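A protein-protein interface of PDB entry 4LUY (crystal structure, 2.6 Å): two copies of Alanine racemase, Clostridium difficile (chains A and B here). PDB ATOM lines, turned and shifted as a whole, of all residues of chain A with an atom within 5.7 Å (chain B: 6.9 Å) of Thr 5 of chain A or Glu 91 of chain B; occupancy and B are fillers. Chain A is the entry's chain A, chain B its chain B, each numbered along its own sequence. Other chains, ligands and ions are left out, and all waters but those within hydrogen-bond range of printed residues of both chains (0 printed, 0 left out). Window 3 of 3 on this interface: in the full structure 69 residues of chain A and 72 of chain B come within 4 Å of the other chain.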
ATOM      1  N   LYS A   3      22.443 -20.507  26.323  1.00  0.00           N
ATOM      2  CA  LYS A   3      22.605 -19.259  27.044  1.00  0.00           C
ATOM      3  C   LYS A   3      23.018 -18.075  26.157  1.00  0.00           C
ATOM      4  O   LYS A   3      22.197 -17.325  25.725  1.00  0.00           O
ATOM      5  CB  LYS A   3      23.610 -19.426  28.166  1.00  0.00           C
ATOM      6  CG  LYS A   3      23.120 -20.154  29.365  1.00  0.00           C
ATOM      7  CD  LYS A   3      22.239 -19.289  30.190  1.00  0.00           C
ATOM      8  CE  LYS A   3      21.360 -20.165  31.034  1.00  0.00           C
ATOM      9  NZ  LYS A   3      20.711 -21.179  30.185  1.00  0.00           N
ATOM     10  N   ILE A   4      24.294 -17.930  25.885  1.00  0.00           N
ATOM     11  CA  ILE A   4      24.772 -16.724  25.254  1.00  0.00           C
ATOM     12  C   ILE A   4      24.575 -16.789  23.758  1.00  0.00           C
ATOM     13  O   ILE A   4      25.266 -17.484  23.063  1.00  0.00           O
ATOM     14  CB  ILE A   4      26.253 -16.517  25.569  1.00  0.00           C
ATOM     15  CG1 ILE A   4      26.440 -16.165  27.016  1.00  0.00           C
ATOM     16  CG2 ILE A   4      26.878 -15.432  24.738  1.00  0.00           C
ATOM     17  CD1 ILE A   4      27.861 -15.869  27.382  1.00  0.00           C
ATOM     18  N   THR A   5      23.625 -16.022  23.284  1.00  0.00           N
ATOM     19  CA  THR A   5      23.332 -15.979  21.893  1.00  0.00           C
ATOM     20  C   THR A   5      24.054 -14.912  21.075  1.00  0.00           C
ATOM     21  O   THR A   5      23.932 -14.911  19.916  1.00  0.00           O
ATOM     22  CB  THR A   5      21.815 -15.963  21.664  1.00  0.00           C
ATOM     23  OG1 THR A   5      21.185 -15.006  22.507  1.00  0.00           O
ATOM     24  CG2 THR A   5      21.266 -17.269  21.988  1.00  0.00           C
ATOM     25  N   VAL A   6      24.795 -14.016  21.702  1.00  0.00           N
ATOM     26  CA  VAL A   6      25.534 -12.963  21.005  1.00  0.00           C
ATOM     27  C   VAL A   6      26.930 -13.352  20.622  1.00  0.00           C
ATOM     28  O   VAL A   6      27.505 -14.191  21.256  1.00  0.00           O
ATOM     29  CB  VAL A   6      25.621 -11.650  21.798  1.00  0.00           C
ATOM     30  CG1 VAL A   6      24.276 -11.137  22.145  1.00  0.00           C
ATOM     31  CG2 VAL A   6      26.491 -11.769  23.012  1.00  0.00           C
ATOM     32  N   PRO A   7      27.469 -12.818  19.560  1.00  0.00           N
ATOM     33  CA  PRO A   7      28.837 -13.121  19.196  1.00  0.00           C
ATOM     34  C   PRO A   7      29.860 -12.564  20.144  1.00  0.00           C
ATOM     35  O   PRO A   7      30.850 -13.152  20.377  1.00  0.00           O
ATOM     36  CB  PRO A   7      28.967 -12.588  17.780  1.00  0.00           C
ATOM     37  CG  PRO A   7      27.801 -11.778  17.561  1.00  0.00           C
ATOM     38  CD  PRO A   7      26.922 -11.773  18.733  1.00  0.00           C
ATOM     39  N   LYS A 253      34.170 -14.356  19.543  1.00  0.00           N
ATOM     40  CA  LYS A 253      34.317 -15.714  19.071  1.00  0.00           C
ATOM     41  C   LYS A 253      34.796 -15.714  17.656  1.00  0.00           C
ATOM     42  O   LYS A 253      34.386 -14.888  16.904  1.00  0.00           O
ATOM     43  CB  LYS A 253      32.963 -16.330  19.015  1.00  0.00           C
ATOM     44  CG  LYS A 253      32.487 -17.034  20.246  1.00  0.00           C
ATOM     45  CD  LYS A 253      30.983 -17.138  20.200  1.00  0.00           C
ATOM     46  CE  LYS A 253      30.505 -18.365  20.921  1.00  0.00           C
ATOM     47  NZ  LYS A 253      30.302 -19.526  20.019  1.00  0.00           N
ATOM     48  N   THR B  67      22.290 -10.445  15.205  1.00  0.00           N
ATOM     49  CA  THR B  67      20.988 -11.047  15.330  1.00  0.00           C
ATOM     50  C   THR B  67      20.059 -10.212  16.199  1.00  0.00           C
ATOM     51  O   THR B  67      18.928  -9.990  15.883  1.00  0.00           O
ATOM     52  CB  THR B  67      21.137 -12.467  15.918  1.00  0.00           C
ATOM     53  OG1 THR B  67      22.057 -13.187  15.145  1.00  0.00           O
ATOM     54  CG2 THR B  67      19.884 -13.214  15.920  1.00  0.00           C
ATOM     55  N   ALA B  68      20.602  -9.753  17.291  1.00  0.00           N
ATOM     56  CA  ALA B  68      19.925  -8.944  18.234  1.00  0.00           C
ATOM     57  C   ALA B  68      19.488  -7.639  17.651  1.00  0.00           C
ATOM     58  O   ALA B  68      18.448  -7.167  17.938  1.00  0.00           O
ATOM     59  CB  ALA B  68      20.818  -8.716  19.385  1.00  0.00           C
ATOM     60  N   TYR B  87      28.203 -12.630  10.623  1.00  0.00           N
ATOM     61  CA  TYR B  87      28.243 -13.928  11.222  1.00  0.00           C
ATOM     62  C   TYR B  87      27.090 -14.170  12.149  1.00  0.00           C
ATOM     63  O   TYR B  87      26.732 -13.311  12.869  1.00  0.00           O
ATOM     64  CB  TYR B  87      29.557 -14.051  11.958  1.00  0.00           C
ATOM     65  CG  TYR B  87      29.695 -15.164  12.941  1.00  0.00           C
ATOM     66  CD1 TYR B  87      29.899 -16.436  12.542  1.00  0.00           C
ATOM     67  CD2 TYR B  87      29.659 -14.926  14.269  1.00  0.00           C
ATOM     68  CE1 TYR B  87      30.034 -17.448  13.449  1.00  0.00           C
ATOM     69  CE2 TYR B  87      29.792 -15.928  15.172  1.00  0.00           C
ATOM     70  CZ  TYR B  87      29.989 -17.190  14.747  1.00  0.00           C
ATOM     71  OH  TYR B  87      30.134 -18.200  15.627  1.00  0.00           O
ATOM     72  N   THR B  88      26.493 -15.340  12.077  1.00  0.00           N
ATOM     73  CA  THR B  88      25.485 -15.762  13.007  1.00  0.00           C
ATOM     74  C   THR B  88      25.949 -17.010  13.740  1.00  0.00           C
ATOM     75  O   THR B  88      26.041 -18.070  13.196  1.00  0.00           O
ATOM     76  CB  THR B  88      24.156 -16.046  12.288  1.00  0.00           C
ATOM     77  OG1 THR B  88      23.722 -14.897  11.612  1.00  0.00           O
ATOM     78  CG2 THR B  88      23.120 -16.412  13.212  1.00  0.00           C
ATOM     79  N   PRO B  89      26.154 -16.899  15.018  1.00  0.00           N
ATOM     80  CA  PRO B  89      26.503 -18.057  15.815  1.00  0.00           C
ATOM     81  C   PRO B  89      25.380 -19.049  15.891  1.00  0.00           C
ATOM     82  O   PRO B  89      24.245 -18.707  15.838  1.00  0.00           O
ATOM     83  CB  PRO B  89      26.784 -17.469  17.185  1.00  0.00           C
ATOM     84  CG  PRO B  89      26.437 -16.048  17.109  1.00  0.00           C
ATOM     85  CD  PRO B  89      26.541 -15.671  15.690  1.00  0.00           C
ATOM     86  N   ASP B  90      25.751 -20.293  16.059  1.00  0.00           N
ATOM     87  CA  ASP B  90      24.884 -21.425  15.947  1.00  0.00           C
ATOM     88  C   ASP B  90      23.766 -21.319  16.938  1.00  0.00           C
ATOM     89  O   ASP B  90      22.678 -21.775  16.763  1.00  0.00           O
ATOM     90  CB  ASP B  90      25.698 -22.672  16.205  1.00  0.00           C
ATOM     91  CG  ASP B  90      26.650 -22.987  15.102  1.00  0.00           C
ATOM     92  OD1 ASP B  90      26.980 -22.146  14.292  1.00  0.00           O
ATOM     93  OD2 ASP B  90      27.101 -24.099  15.053  1.00  0.00           O
ATOM     94  N   GLU B  91      24.098 -20.642  17.988  1.00  0.00           N
ATOM     95  CA  GLU B  91      23.225 -20.401  19.069  1.00  0.00           C
ATOM     96  C   GLU B  91      22.165 -19.421  18.752  1.00  0.00           C
ATOM     97  O   GLU B  91      21.263 -19.279  19.479  1.00  0.00           O
ATOM     98  CB  GLU B  91      24.065 -19.962  20.226  1.00  0.00           C
ATOM     99  CG  GLU B  91      24.993 -21.076  20.623  1.00  0.00           C
ATOM    100  CD  GLU B  91      26.426 -20.852  20.257  1.00  0.00           C
ATOM    101  OE1 GLU B  91      26.767 -20.562  19.135  1.00  0.00           O
ATOM    102  OE2 GLU B  91      27.238 -20.986  21.139  1.00  0.00           O
ATOM    103  N   ALA B  92      22.300 -18.728  17.654  1.00  0.00           N
ATOM    104  CA  ALA B  92      21.322 -17.763  17.274  1.00  0.00           C
ATOM    105  C   ALA B  92      20.490 -18.139  16.095  1.00  0.00           C
ATOM    106  O   ALA B  92      19.623 -17.432  15.734  1.00  0.00           O
ATOM    107  CB  ALA B  92      21.980 -16.446  17.037  1.00  0.00           C
ATOM    108  N   PHE B  93      20.740 -19.284  15.531  1.00  0.00           N
ATOM    109  CA  PHE B  93      20.078 -19.680  14.342  1.00  0.00           C
ATOM    110  C   PHE B  93      18.608 -19.769  14.530  1.00  0.00           C
ATOM    111  O   PHE B  93      17.879 -19.315  13.733  1.00  0.00           O
ATOM    112  CB  PHE B  93      20.495 -21.085  14.013  1.00  0.00           C
ATOM    113  CG  PHE B  93      21.834 -21.219  13.427  1.00  0.00           C
ATOM    114  CD1 PHE B  93      22.517 -20.171  12.948  1.00  0.00           C
ATOM    115  CD2 PHE B  93      22.386 -22.432  13.354  1.00  0.00           C
ATOM    116  CE1 PHE B  93      23.724 -20.338  12.410  1.00  0.00           C
ATOM    117  CE2 PHE B  93      23.580 -22.610  12.811  1.00  0.00           C
ATOM    118  CZ  PHE B  93      24.262 -21.562  12.359  1.00  0.00           C
ATOM    119  N   GLU B  94      18.188 -20.411  15.585  1.00  0.00           N
ATOM    120  CA  GLU B  94      16.800 -20.614  15.825  1.00  0.00           C
ATOM    121  C   GLU B  94      16.014 -19.340  16.025  1.00  0.00           C
ATOM    122  O   GLU B  94      14.961 -19.182  15.469  1.00  0.00           O
ATOM    123  CB  GLU B  94      16.639 -21.523  17.012  1.00  0.00           C
ATOM    124  CG  GLU B  94      15.221 -21.714  17.457  1.00  0.00           C
ATOM    125  CD  GLU B  94      15.093 -22.544  18.672  1.00  0.00           C
ATOM    126  OE1 GLU B  94      14.993 -23.756  18.598  1.00  0.00           O
ATOM    127  OE2 GLU B  94      15.075 -21.959  19.724  1.00  0.00           O
ATOM    128  N   ASP B  95      16.547 -18.427  16.807  1.00  0.00           N
ATOM    129  CA  ASP B  95      15.976 -17.130  16.965  1.00  0.00           C
ATOM    130  C   ASP B  95      15.955 -16.362  15.674  1.00  0.00           C
ATOM    131  O   ASP B  95      15.068 -15.597  15.476  1.00  0.00           O
ATOM    132  CB  ASP B  95      16.681 -16.346  18.036  1.00  0.00           C
ATOM    133  CG  ASP B  95      16.387 -16.846  19.410  1.00  0.00           C
ATOM    134  OD1 ASP B  95      15.420 -17.569  19.582  1.00  0.00           O
ATOM    135  OD2 ASP B  95      17.135 -16.523  20.335  1.00  0.00           O
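No position is printed for both chains.
Among the printed residues, pairs that only touch across the chains: Thr 5 of chain A with Glu 91 of chain B (3.2 Å), Thr 5 of chain A with Ala 92 of chain B (3.8 Å), Thr 5 of chain A with Pro 89 of chain B (3.9 Å) and Ile 4 of chain A with Glu 91 of chain B (3.95 Å).
Printed residues of chain A that touch a printed residue of chain B: Ile 4, Thr 5 and Lys 253. Hydrophobic or aromatic side chains of chain B within 4 Å of the printed part of chain A: Pro 89 and Ala 92. Along chain B the printed residues that touch a printed residue of chain A span positions 89 to 92. Among the printed residues, 5 pairs touch across the chains.
NZ of Lys 253 of chain A is in salt-bridge range of OE2 of Glu 91 of chain B, at 3.6 Å.
Of the printed residues of chain B, Thr 5 of chain A touches Pro 89, Glu 91 and Ala 92. Glu 91 of chain B touches three residues of chain A. Of the printed residues of chain B, Lys 253 of chain A touches Glu 91 (3.6 Å). Printed residues of chain A within 4 Å of Ala 92 of chain B: Thr 5. Asp 95 of chain B touches none of the printed residues of chain A. Glu 94 of chain B touches none of the printed residues of chain A. The nearest printed residue of chain B that does not touch Ile 4 of chain A is Pro 89 of chain B (6.1 Å).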
